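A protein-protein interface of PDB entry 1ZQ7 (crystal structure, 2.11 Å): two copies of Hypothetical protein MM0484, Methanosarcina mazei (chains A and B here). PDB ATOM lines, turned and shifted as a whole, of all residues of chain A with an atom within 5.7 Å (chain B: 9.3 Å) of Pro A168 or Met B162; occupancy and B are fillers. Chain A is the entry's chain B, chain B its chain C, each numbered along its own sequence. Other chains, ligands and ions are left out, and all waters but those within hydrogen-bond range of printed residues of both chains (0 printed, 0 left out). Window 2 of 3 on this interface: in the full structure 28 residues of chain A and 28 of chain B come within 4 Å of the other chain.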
ATOM      1  N   ASP A 155      18.822  30.031   2.108  1.00  0.00           N
ATOM      2  CA  ASP A 155      19.342  29.048   1.169  1.00  0.00           C
ATOM      3  C   ASP A 155      18.683  27.692   1.406  1.00  0.00           C
ATOM      4  O   ASP A 155      18.213  27.039   0.473  1.00  0.00           O
ATOM      5  CB  ASP A 155      20.859  28.880   1.334  1.00  0.00           C
ATOM      6  CG  ASP A 155      21.643  30.153   1.027  1.00  0.00           C
ATOM      7  OD1 ASP A 155      21.368  30.815  -0.001  1.00  0.00           O
ATOM      8  OD2 ASP A 155      22.561  30.477   1.809  1.00  0.00           O
ATOM      9  N   LEU A 157      15.837  26.811   2.825  1.00  0.00           N
ATOM     10  CA  LEU A 157      14.437  26.758   2.435  1.00  0.00           C
ATOM     11  C   LEU A 157      14.350  26.583   0.924  1.00  0.00           C
ATOM     12  O   LEU A 157      13.611  25.730   0.429  1.00  0.00           O
ATOM     13  CB  LEU A 157      13.732  28.053   2.859  1.00  0.00           C
ATOM     14  CG  LEU A 157      13.472  28.182   4.365  1.00  0.00           C
ATOM     15  CD1 LEU A 157      13.331  29.646   4.748  1.00  0.00           C
ATOM     16  CD2 LEU A 157      12.220  27.405   4.732  1.00  0.00           C
ATOM     17  N   SER A 158      15.128  27.380   0.195  1.00  0.00           N
ATOM     18  CA  SER A 158      15.124  27.323  -1.261  1.00  0.00           C
ATOM     19  C   SER A 158      15.598  25.979  -1.822  1.00  0.00           C
ATOM     20  O   SER A 158      14.971  25.441  -2.730  1.00  0.00           O
ATOM     21  CB  SER A 158      15.963  28.471  -1.831  1.00  0.00           C
ATOM     22  OG  SER A 158      15.360  29.718  -1.502  1.00  0.00           O
ATOM     23  N   HIS A 159      16.694  25.433  -1.304  1.00  0.00           N
ATOM     24  CA  HIS A 159      17.155  24.138  -1.808  1.00  0.00           C
ATOM     25  C   HIS A 159      16.152  23.031  -1.497  1.00  0.00           C
ATOM     26  O   HIS A 159      15.899  22.160  -2.328  1.00  0.00           O
ATOM     27  CB  HIS A 159      18.521  23.772  -1.231  1.00  0.00           C
ATOM     28  CG  HIS A 159      19.669  24.393  -1.969  1.00  0.00           C
ATOM     29  ND1 HIS A 159      20.096  25.677  -1.730  1.00  0.00           N
ATOM     30  CD2 HIS A 159      20.440  23.910  -2.969  1.00  0.00           C
ATOM     31  CE1 HIS A 159      21.094  25.964  -2.559  1.00  0.00           C
ATOM     32  NE2 HIS A 159      21.317  24.914  -3.316  1.00  0.00           N
ATOM     33  N   CYS A 161      13.015  23.343  -1.283  1.00  0.00           N
ATOM     34  CA  CYS A 161      11.898  23.483  -2.207  1.00  0.00           C
ATOM     35  C   CYS A 161      12.243  22.808  -3.531  1.00  0.00           C
ATOM     36  O   CYS A 161      11.442  22.049  -4.063  1.00  0.00           O
ATOM     37  CB  CYS A 161      11.561  24.954  -2.450  1.00  0.00           C
ATOM     38  SG  CYS A 161      10.616  25.695  -1.118  1.00  0.00           S
ATOM     39  N   MET A 162      13.432  23.078  -4.062  1.00  0.00           N
ATOM     40  CA  MET A 162      13.822  22.459  -5.324  1.00  0.00           C
ATOM     41  C   MET A 162      13.979  20.954  -5.165  1.00  0.00           C
ATOM     42  O   MET A 162      13.764  20.200  -6.111  1.00  0.00           O
ATOM     43  CB  MET A 162      15.122  23.062  -5.860  1.00  0.00           C
ATOM     44  CG  MET A 162      15.497  22.520  -7.232  1.00  0.00           C
ATOM     45  SD  MET A 162      16.713  23.644  -8.215  1.00  0.00           S
ATOM     46  CE  MET A 162      18.410  22.950  -7.513  1.00  0.00           C
ATOM     47  N   LEU A 166       9.898  21.601  -6.568  1.00  0.00           N
ATOM     48  CA  LEU A 166       9.193  22.864  -6.708  1.00  0.00           C
ATOM     49  C   LEU A 166      10.157  23.993  -7.027  1.00  0.00           C
ATOM     50  O   LEU A 166      11.379  23.808  -7.064  1.00  0.00           O
ATOM     51  CB  LEU A 166       8.446  23.201  -5.414  1.00  0.00           C
ATOM     52  CG  LEU A 166       7.405  22.176  -4.965  1.00  0.00           C
ATOM     53  CD1 LEU A 166       7.018  22.435  -3.518  1.00  0.00           C
ATOM     54  CD2 LEU A 166       6.188  22.248  -5.881  1.00  0.00           C
ATOM     55  N   SER A 167       9.583  25.167  -7.266  1.00  0.00           N
ATOM     56  CA  SER A 167      10.366  26.348  -7.555  1.00  0.00           C
ATOM     57  C   SER A 167      11.059  26.757  -6.270  1.00  0.00           C
ATOM     58  O   SER A 167      10.483  26.657  -5.188  1.00  0.00           O
ATOM     59  CB  SER A 167       9.460  27.494  -8.021  1.00  0.00           C
ATOM     60  OG  SER A 167      10.203  28.701  -8.123  1.00  0.00           O
ATOM     61  N   PRO A 168      12.312  27.213  -6.370  1.00  0.00           N
ATOM     62  CA  PRO A 168      13.079  27.643  -5.200  1.00  0.00           C
ATOM     63  C   PRO A 168      12.288  28.617  -4.316  1.00  0.00           C
ATOM     64  O   PRO A 168      12.395  28.571  -3.091  1.00  0.00           O
ATOM     65  CB  PRO A 168      14.303  28.311  -5.817  1.00  0.00           C
ATOM     66  CG  PRO A 168      14.509  27.549  -7.065  1.00  0.00           C
ATOM     67  CD  PRO A 168      13.114  27.311  -7.599  1.00  0.00           C
ATOM     68  N   ASP A 169      11.491  29.486  -4.938  1.00  0.00           N
ATOM     69  CA  ASP A 169      10.714  30.476  -4.188  1.00  0.00           C
ATOM     70  C   ASP A 169       9.362  29.993  -3.670  1.00  0.00           C
ATOM     71  O   ASP A 169       8.596  30.772  -3.105  1.00  0.00           O
ATOM     72  CB  ASP A 169      10.514  31.752  -5.030  1.00  0.00           C
ATOM     73  CG  ASP A 169       9.527  31.560  -6.169  1.00  0.00           C
ATOM     74  OD1 ASP A 169       9.043  30.428  -6.373  1.00  0.00           O
ATOM     75  OD2 ASP A 169       9.231  32.552  -6.867  1.00  0.00           O
ATOM     76  N   ALA A 170       9.069  28.708  -3.846  1.00  0.00           N
ATOM     77  CA  ALA A 170       7.803  28.156  -3.378  1.00  0.00           C
ATOM     78  C   ALA A 170       7.531  28.470  -1.906  1.00  0.00           C
ATOM     79  O   ALA A 170       6.377  28.688  -1.520  1.00  0.00           O
ATOM     80  CB  ALA A 170       7.773  26.654  -3.608  1.00  0.00           C
ATOM     81  N   TRP A 171       8.573  28.505  -1.077  1.00  0.00           N
ATOM     82  CA  TRP A 171       8.343  28.801   0.335  1.00  0.00           C
ATOM     83  C   TRP A 171       7.893  30.247   0.515  1.00  0.00           C
ATOM     84  O   TRP A 171       7.126  30.571   1.424  1.00  0.00           O
ATOM     85  CB  TRP A 171       9.596  28.549   1.178  1.00  0.00           C
ATOM     86  CG  TRP A 171      10.791  29.388   0.836  1.00  0.00           C
ATOM     87  CD1 TRP A 171      11.749  29.112  -0.101  1.00  0.00           C
ATOM     88  CD2 TRP A 171      11.189  30.612   1.469  1.00  0.00           C
ATOM     89  NE1 TRP A 171      12.727  30.085  -0.084  1.00  0.00           N
ATOM     90  CE2 TRP A 171      12.410  31.016   0.874  1.00  0.00           C
ATOM     91  CE3 TRP A 171      10.641  31.406   2.490  1.00  0.00           C
ATOM     92  CZ2 TRP A 171      13.089  32.176   1.257  1.00  0.00           C
ATOM     93  CZ3 TRP A 171      11.318  32.563   2.875  1.00  0.00           C
ATOM     94  CH2 TRP A 171      12.531  32.934   2.260  1.00  0.00           C
ATOM     95  N   VAL A 172       8.376  31.113  -0.364  1.00  0.00           N
ATOM     96  CA  VAL A 172       8.026  32.517  -0.311  1.00  0.00           C
ATOM     97  C   VAL A 172       6.544  32.685  -0.633  1.00  0.00           C
ATOM     98  O   VAL A 172       5.919  33.639  -0.195  1.00  0.00           O
ATOM     99  CB  VAL A 172       8.855  33.319  -1.323  1.00  0.00           C
ATOM    100  CG1 VAL A 172       8.661  34.816  -1.096  1.00  0.00           C
ATOM    101  CG2 VAL A 172      10.324  32.937  -1.198  1.00  0.00           C
ATOM    102  N   VAL B 132      30.750  24.692  -9.310  1.00  0.00           N
ATOM    103  CA  VAL B 132      30.223  25.340 -10.506  1.00  0.00           C
ATOM    104  C   VAL B 132      30.853  26.722 -10.547  1.00  0.00           C
ATOM    105  O   VAL B 132      30.825  27.458  -9.554  1.00  0.00           O
ATOM    106  CB  VAL B 132      28.684  25.481 -10.480  1.00  0.00           C
ATOM    107  CG1 VAL B 132      28.226  26.375 -11.627  1.00  0.00           C
ATOM    108  CG2 VAL B 132      28.029  24.097 -10.607  1.00  0.00           C
ATOM    109  N   CYS B 137      31.764  34.166  -9.897  1.00  0.00           N
ATOM    110  CA  CYS B 137      30.828  33.454  -9.022  1.00  0.00           C
ATOM    111  C   CYS B 137      31.213  31.976  -8.957  1.00  0.00           C
ATOM    112  O   CYS B 137      31.535  31.363  -9.969  1.00  0.00           O
ATOM    113  CB  CYS B 137      29.386  33.579  -9.538  1.00  0.00           C
ATOM    114  SG  CYS B 137      28.560  35.176  -9.227  1.00  0.00           S
ATOM    115  N   GLN B 138      31.166  31.400  -7.765  1.00  0.00           N
ATOM    116  CA  GLN B 138      31.532  30.002  -7.601  1.00  0.00           C
ATOM    117  C   GLN B 138      30.791  29.385  -6.420  1.00  0.00           C
ATOM    118  O   GLN B 138      30.526  30.050  -5.424  1.00  0.00           O
ATOM    119  CB  GLN B 138      33.050  29.912  -7.405  1.00  0.00           C
ATOM    120  CG  GLN B 138      33.633  28.521  -7.475  1.00  0.00           C
ATOM    121  CD  GLN B 138      35.138  28.532  -7.724  1.00  0.00           C
ATOM    122  OE1 GLN B 138      35.803  27.500  -7.630  1.00  0.00           O
ATOM    123  NE2 GLN B 138      35.678  29.702  -8.050  1.00  0.00           N
ATOM    124  N   GLY B 139      30.439  28.111  -6.546  1.00  0.00           N
ATOM    125  CA  GLY B 139      29.741  27.432  -5.471  1.00  0.00           C
ATOM    126  C   GLY B 139      30.125  25.969  -5.422  1.00  0.00           C
ATOM    127  O   GLY B 139      30.443  25.377  -6.451  1.00  0.00           O
ATOM    128  N   LEU B 140      30.117  25.371  -4.235  1.00  0.00           N
ATOM    129  CA  LEU B 140      30.456  23.961  -4.160  1.00  0.00           C
ATOM    130  C   LEU B 140      29.616  23.179  -3.174  1.00  0.00           C
ATOM    131  O   LEU B 140      29.094  23.718  -2.189  1.00  0.00           O
ATOM    132  CB  LEU B 140      31.952  23.772  -3.853  1.00  0.00           C
ATOM    133  CG  LEU B 140      32.582  23.676  -2.457  1.00  0.00           C
ATOM    134  CD1 LEU B 140      32.036  22.473  -1.657  1.00  0.00           C
ATOM    135  CD2 LEU B 140      34.101  23.521  -2.644  1.00  0.00           C
ATOM    136  N   LEU B 141      29.472  21.896  -3.469  1.00  0.00           N
ATOM    137  CA  LEU B 141      28.723  20.990  -2.614  1.00  0.00           C
ATOM    138  C   LEU B 141      29.590  19.753  -2.416  1.00  0.00           C
ATOM    139  O   LEU B 141      30.206  19.235  -3.364  1.00  0.00           O
ATOM    140  CB  LEU B 141      27.368  20.640  -3.246  1.00  0.00           C
ATOM    141  CG  LEU B 141      26.359  21.801  -3.253  1.00  0.00           C
ATOM    142  CD1 LEU B 141      25.099  21.416  -4.018  1.00  0.00           C
ATOM    143  CD2 LEU B 141      26.018  22.185  -1.819  1.00  0.00           C
ATOM    144  N   MET B 151      19.732  12.636  -4.328  1.00  0.00           N
ATOM    145  CA  MET B 151      19.823  13.479  -5.519  1.00  0.00           C
ATOM    146  C   MET B 151      20.506  12.691  -6.632  1.00  0.00           C
ATOM    147  O   MET B 151      21.445  11.946  -6.357  1.00  0.00           O
ATOM    148  CB  MET B 151      20.676  14.718  -5.256  1.00  0.00           C
ATOM    149  CG  MET B 151      20.249  15.629  -4.140  1.00  0.00           C
ATOM    150  SD  MET B 151      21.484  17.131  -4.156  1.00  0.00           S
ATOM    151  CE  MET B 151      20.538  18.279  -2.913  1.00  0.00           C
ATOM    152  N   ILE B 154      21.447  15.095 -12.273  1.00  0.00           N
ATOM    153  CA  ILE B 154      20.748  16.316 -12.658  1.00  0.00           C
ATOM    154  C   ILE B 154      20.478  17.193 -11.439  1.00  0.00           C
ATOM    155  O   ILE B 154      20.720  18.395 -11.477  1.00  0.00           O
ATOM    156  CB  ILE B 154      19.430  15.978 -13.383  1.00  0.00           C
ATOM    157  CG1 ILE B 154      19.756  15.370 -14.751  1.00  0.00           C
ATOM    158  CG2 ILE B 154      18.562  17.229 -13.517  1.00  0.00           C
ATOM    159  CD1 ILE B 154      18.679  14.448 -15.295  1.00  0.00           C
ATOM    160  N   ASP B 155      19.990  16.598 -10.353  1.00  0.00           N
ATOM    161  CA  ASP B 155      19.731  17.372  -9.139  1.00  0.00           C
ATOM    162  C   ASP B 155      21.021  18.028  -8.635  1.00  0.00           C
ATOM    163  O   ASP B 155      21.063  19.225  -8.377  1.00  0.00           O
ATOM    164  CB  ASP B 155      19.173  16.485  -8.016  1.00  0.00           C
ATOM    165  CG  ASP B 155      17.876  15.786  -8.394  1.00  0.00           C
ATOM    166  OD1 ASP B 155      17.050  16.395  -9.101  1.00  0.00           O
ATOM    167  OD2 ASP B 155      17.675  14.628  -7.963  1.00  0.00           O
ATOM    168  N   PHE B 156      22.075  17.235  -8.488  1.00  0.00           N
ATOM    169  CA  PHE B 156      23.349  17.747  -7.991  1.00  0.00           C
ATOM    170  C   PHE B 156      23.849  18.935  -8.806  1.00  0.00           C
ATOM    171  O   PHE B 156      24.292  19.933  -8.237  1.00  0.00           O
ATOM    172  CB  PHE B 156      24.393  16.626  -7.991  1.00  0.00           C
ATOM    173  CG  PHE B 156      25.416  16.739  -6.889  1.00  0.00           C
ATOM    174  CD1 PHE B 156      25.126  17.425  -5.711  1.00  0.00           C
ATOM    175  CD2 PHE B 156      26.657  16.121  -7.015  1.00  0.00           C
ATOM    176  CE1 PHE B 156      26.048  17.475  -4.665  1.00  0.00           C
ATOM    177  CE2 PHE B 156      27.588  16.163  -5.979  1.00  0.00           C
ATOM    178  CZ  PHE B 156      27.289  16.845  -4.803  1.00  0.00           C
ATOM    179  N   LEU B 157      23.790  18.829 -10.130  1.00  0.00           N
ATOM    180  CA  LEU B 157      24.241  19.926 -10.994  1.00  0.00           C
ATOM    181  C   LEU B 157      23.389  21.175 -10.757  1.00  0.00           C
ATOM    182  O   LEU B 157      23.913  22.285 -10.640  1.00  0.00           O
ATOM    183  CB  LEU B 157      24.149  19.516 -12.462  1.00  0.00           C
ATOM    184  CG  LEU B 157      25.172  18.497 -12.990  1.00  0.00           C
ATOM    185  CD1 LEU B 157      24.603  17.815 -14.218  1.00  0.00           C
ATOM    186  CD2 LEU B 157      26.494  19.177 -13.322  1.00  0.00           C
ATOM    187  N   SER B 158      22.075  20.989 -10.674  1.00  0.00           N
ATOM    188  CA  SER B 158      21.164  22.113 -10.463  1.00  0.00           C
ATOM    189  C   SER B 158      21.370  22.734  -9.092  1.00  0.00           C
ATOM    190  O   SER B 158      21.419  23.960  -8.967  1.00  0.00           O
ATOM    191  CB  SER B 158      19.703  21.660 -10.595  1.00  0.00           C
ATOM    192  OG  SER B 158      19.420  21.189 -11.902  1.00  0.00           O
ATOM    193  N   HIS B 159      21.489  21.895  -8.059  1.00  0.00           N
ATOM    194  CA  HIS B 159      21.674  22.423  -6.713  1.00  0.00           C
ATOM    195  C   HIS B 159      23.015  23.148  -6.561  1.00  0.00           C
ATOM    196  O   HIS B 159      23.081  24.196  -5.920  1.00  0.00           O
ATOM    197  CB  HIS B 159      21.541  21.318  -5.656  1.00  0.00           C
ATOM    198  CG  HIS B 159      20.120  20.944  -5.340  1.00  0.00           C
ATOM    199  ND1 HIS B 159      19.415  20.014  -6.070  1.00  0.00           N
ATOM    200  CD2 HIS B 159      19.278  21.384  -4.372  1.00  0.00           C
ATOM    201  CE1 HIS B 159      18.197  19.891  -5.565  1.00  0.00           C
ATOM    202  NE2 HIS B 159      18.090  20.710  -4.537  1.00  0.00           N
ATOM    203  N   THR B 160      24.080  22.611  -7.157  1.00  0.00           N
ATOM    204  CA  THR B 160      25.376  23.263  -7.044  1.00  0.00           C
ATOM    205  C   THR B 160      25.353  24.623  -7.743  1.00  0.00           C
ATOM    206  O   THR B 160      26.028  25.560  -7.310  1.00  0.00           O
ATOM    207  CB  THR B 160      26.526  22.397  -7.632  1.00  0.00           C
ATOM    208  OG1 THR B 160      26.546  21.114  -6.987  1.00  0.00           O
ATOM    209  CG2 THR B 160      27.857  23.066  -7.378  1.00  0.00           C
ATOM    210  N   CYS B 161      24.578  24.735  -8.819  1.00  0.00           N
ATOM    211  CA  CYS B 161      24.484  26.008  -9.534  1.00  0.00           C
ATOM    212  C   CYS B 161      23.821  27.053  -8.657  1.00  0.00           C
ATOM    213  O   CYS B 161      24.259  28.206  -8.623  1.00  0.00           O
ATOM    214  CB  CYS B 161      23.687  25.866 -10.835  1.00  0.00           C
ATOM    215  SG  CYS B 161      24.608  25.078 -12.167  1.00  0.00           S
ATOM    216  N   MET B 162      22.767  26.658  -7.946  1.00  0.00           N
ATOM    217  CA  MET B 162      22.076  27.598  -7.078  1.00  0.00           C
ATOM    218  C   MET B 162      22.987  27.935  -5.905  1.00  0.00           C
ATOM    219  O   MET B 162      22.986  29.059  -5.424  1.00  0.00           O
ATOM    220  CB  MET B 162      20.742  27.025  -6.581  1.00  0.00           C
ATOM    221  CG  MET B 162      19.941  28.027  -5.745  1.00  0.00           C
ATOM    222  SD  MET B 162      18.008  27.713  -5.768  1.00  0.00           S
ATOM    223  CE  MET B 162      17.924  26.211  -4.543  1.00  0.00           C
ATOM    224  N   LYS B 163      23.774  26.959  -5.458  1.00  0.00           N
ATOM    225  CA  LYS B 163      24.715  27.182  -4.362  1.00  0.00           C
ATOM    226  C   LYS B 163      25.705  28.270  -4.775  1.00  0.00           C
ATOM    227  O   LYS B 163      26.241  28.987  -3.941  1.00  0.00           O
ATOM    228  CB  LYS B 163      25.491  25.897  -4.045  1.00  0.00           C
ATOM    229  CG  LYS B 163      26.418  26.015  -2.840  1.00  0.00           C
ATOM    230  CD  LYS B 163      25.614  26.188  -1.560  1.00  0.00           C
ATOM    231  CE  LYS B 163      25.977  27.470  -0.827  1.00  0.00           C
ATOM    232  NZ  LYS B 163      27.393  27.489  -0.370  1.00  0.00           N
ATOM    233  N   ALA B 164      25.960  28.376  -6.072  1.00  0.00           N
ATOM    234  CA  ALA B 164      26.883  29.377  -6.590  1.00  0.00           C
ATOM    235  C   ALA B 164      26.194  30.740  -6.741  1.00  0.00           C
ATOM    236  O   ALA B 164      26.832  31.723  -7.101  1.00  0.00           O
ATOM    237  CB  ALA B 164      27.437  28.922  -7.934  1.00  0.00           C
ATOM    238  N   GLY B 165      24.898  30.788  -6.445  1.00  0.00           N
ATOM    239  CA  GLY B 165      24.145  32.031  -6.572  1.00  0.00           C
ATOM    240  C   GLY B 165      23.596  32.180  -7.980  1.00  0.00           C
ATOM    241  O   GLY B 165      23.045  33.218  -8.347  1.00  0.00           O
ATOM    242  N   LEU B 166      23.724  31.118  -8.767  1.00  0.00           N
ATOM    243  CA  LEU B 166      23.284  31.130 -10.156  1.00  0.00           C
ATOM    244  C   LEU B 166      21.968  30.395 -10.341  1.00  0.00           C
ATOM    245  O   LEU B 166      21.491  29.713  -9.434  1.00  0.00           O
ATOM    246  CB  LEU B 166      24.354  30.471 -11.039  1.00  0.00           C
ATOM    247  CG  LEU B 166      25.786  31.009 -10.935  1.00  0.00           C
ATOM    248  CD1 LEU B 166      26.742  30.113 -11.736  1.00  0.00           C
ATOM    249  CD2 LEU B 166      25.840  32.441 -11.458  1.00  0.00           C
ATOM    250  N   SER B 167      21.379  30.539 -11.523  1.00  0.00           N
ATOM    251  CA  SER B 167      20.129  29.861 -11.827  1.00  0.00           C
ATOM    252  C   SER B 167      20.423  28.369 -11.891  1.00  0.00           C
ATOM    253  O   SER B 167      21.520  27.969 -12.263  1.00  0.00           O
ATOM    254  CB  SER B 167      19.577  30.334 -13.171  1.00  0.00           C
ATOM    255  OG  SER B 167      18.498  29.514 -13.590  1.00  0.00           O
ATOM    256  N   PRO B 168      19.440  27.528 -11.535  1.00  0.00           N
ATOM    257  CA  PRO B 168      19.584  26.073 -11.547  1.00  0.00           C
ATOM    258  C   PRO B 168      19.937  25.509 -12.916  1.00  0.00           C
ATOM    259  O   PRO B 168      20.530  24.431 -13.015  1.00  0.00           O
ATOM    260  CB  PRO B 168      18.218  25.591 -11.069  1.00  0.00           C
ATOM    261  CG  PRO B 168      17.760  26.698 -10.176  1.00  0.00           C
ATOM    262  CD  PRO B 168      18.128  27.911 -10.981  1.00  0.00           C
ATOM    263  N   ASP B 169      19.587  26.226 -13.979  1.00  0.00           N
ATOM    264  CA  ASP B 169      19.877  25.720 -15.311  1.00  0.00           C
ATOM    265  C   ASP B 169      21.176  26.275 -15.899  1.00  0.00           C
ATOM    266  O   ASP B 169      21.462  26.084 -17.082  1.00  0.00           O
ATOM    267  CB  ASP B 169      18.691  25.997 -16.251  1.00  0.00           C
ATOM    268  CG  ASP B 169      18.547  27.463 -16.611  1.00  0.00           C
ATOM    269  OD1 ASP B 169      19.170  28.317 -15.948  1.00  0.00           O
ATOM    270  OD2 ASP B 169      17.796  27.766 -17.564  1.00  0.00           O
ATOM    271  N   ALA B 170      21.963  26.944 -15.067  1.00  0.00           N
ATOM    272  CA  ALA B 170      23.228  27.517 -15.512  1.00  0.00           C
ATOM    273  C   ALA B 170      24.129  26.459 -16.143  1.00  0.00           C
ATOM    274  O   ALA B 170      24.829  26.740 -17.107  1.00  0.00           O
ATOM    275  CB  ALA B 170      23.943  28.191 -14.343  1.00  0.00           C
ATOM    276  N   TRP B 171      24.111  25.240 -15.608  1.00  0.00           N
ATOM    277  CA  TRP B 171      24.945  24.180 -16.182  1.00  0.00           C
ATOM    278  C   TRP B 171      24.426  23.772 -17.557  1.00  0.00           C
ATOM    279  O   TRP B 171      25.189  23.309 -18.406  1.00  0.00           O
ATOM    280  CB  TRP B 171      24.987  22.942 -15.275  1.00  0.00           C
ATOM    281  CG  TRP B 171      23.673  22.249 -15.063  1.00  0.00           C
ATOM    282  CD1 TRP B 171      22.765  22.497 -14.067  1.00  0.00           C
ATOM    283  CD2 TRP B 171      23.135  21.156 -15.831  1.00  0.00           C
ATOM    284  NE1 TRP B 171      21.708  21.623 -14.165  1.00  0.00           N
ATOM    285  CE2 TRP B 171      21.909  20.789 -15.234  1.00  0.00           C
ATOM    286  CE3 TRP B 171      23.578  20.444 -16.961  1.00  0.00           C
ATOM    287  CZ2 TRP B 171      21.113  19.748 -15.728  1.00  0.00           C
ATOM    288  CZ3 TRP B 171      22.789  19.408 -17.452  1.00  0.00           C
ATOM    289  CH2 TRP B 171      21.568  19.069 -16.830  1.00  0.00           C
ATOM    290  N   ALA B 175      27.667  26.603 -18.146  1.00  0.00           N
ATOM    291  CA  ALA B 175      28.452  27.065 -17.007  1.00  0.00           C
ATOM    292  C   ALA B 175      29.520  26.004 -16.704  1.00  0.00           C
ATOM    293  O   ALA B 175      29.280  24.810 -16.876  1.00  0.00           O
ATOM    294  CB  ALA B 175      27.551  27.263 -15.799  1.00  0.00           C
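OG of Ser A158 is in hydrogen-bond range of NE1 of Trp A171. The side-chain hydroxyl (OG) of Ser B158 is in hydrogen-bond range of the indole nitrogen (NE1) of Trp B171 (3.2 Å). The indole nitrogen (NE1) of Trp B171 sits close to the backbone carbonyl oxygen (O) of Pro B168 (3.3 Å). O of Asp B155 is in hydrogen-bond range of ND1 of His B159 (2.9 Å). The backbone carbonyl oxygen (O) of Ile B154 is in hydrogen-bond range of the side-chain hydroxyl (OG) of Ser B158. The backbone carbonyl oxygen (O) of Asp A155 is in hydrogen-bond range of a ring nitrogen (ND1) of His A159, 3.2 Å away.
The backbone carbonyl oxygen (O) of His B159 is in hydrogen-bond range of a ring nitrogen (NE2) of His A159 (3.2 Å).
Ser A158 touches Met B162. Met B162 touches His A159 (CE to CA, 3.5 Å). His A159 touches Lys B163. CE of Met A162 touches C of Ser B158 (3.4 Å). His B159 touches Met A162 (N to CE, 3.3 Å). Pro B168 touches Met A162 (CB to SD, 3.8 Å). Met B162 touches Pro A168.
Asp A155 touches none of the printed residues of chain B. Ser A158 touches just one residue of chain B: Met B162 (3.5 Å). His A159 touches three residues of chain B. Printed residues of chain B within 4 Å of Met A162: Ser B158 (3.4 Å), His B159 (3.3 Å) and Pro B168 (3.8 Å). Ser A167 touches none of the printed residues of chain B. Of chain B, only Met B162 (3.7 Å) comes within 4 Å of Pro A168. Of the printed residues of chain A, His B159 touches His A159 (3.1 Å) and Met A162 (3.3 Å). Met B162 touches three residues of chain A. The nearest residue of chain A that does not touch Met B162 is Met A162 (4.4 Å).
Ser A158 touches Met B162, and with the chains exchanged Met A162 touches Ser B158. His A159 touches its own counterpart, His B159. His A159 touches Met B162, and with the chains exchanged Met A162 touches His B159. Met A162 touches Pro B168, and with the chains exchanged Pro A168 touches Met B162. Positions printed for both chains: 155, 157, 158, 159, 161, 162, 166, 167, 168, 169, 170 and 171. Of the 8 pairs that touch across the chains among the printed residues, 7 have their exchanged pair printed and touching as well.
Of the 26 printed residues of chain B, 5 touch a printed residue of chain A. Hydrophobic or aromatic side chains of chain A that line the printed part of chain B: His A159, Met A162 and Pro A168. Among the printed residues, 8 pairs touch across the chains. Among the printed residues, no Asp or Glu carboxylate lies within 4 Å of a Lys or Arg side-chain nitrogen of the other chain.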
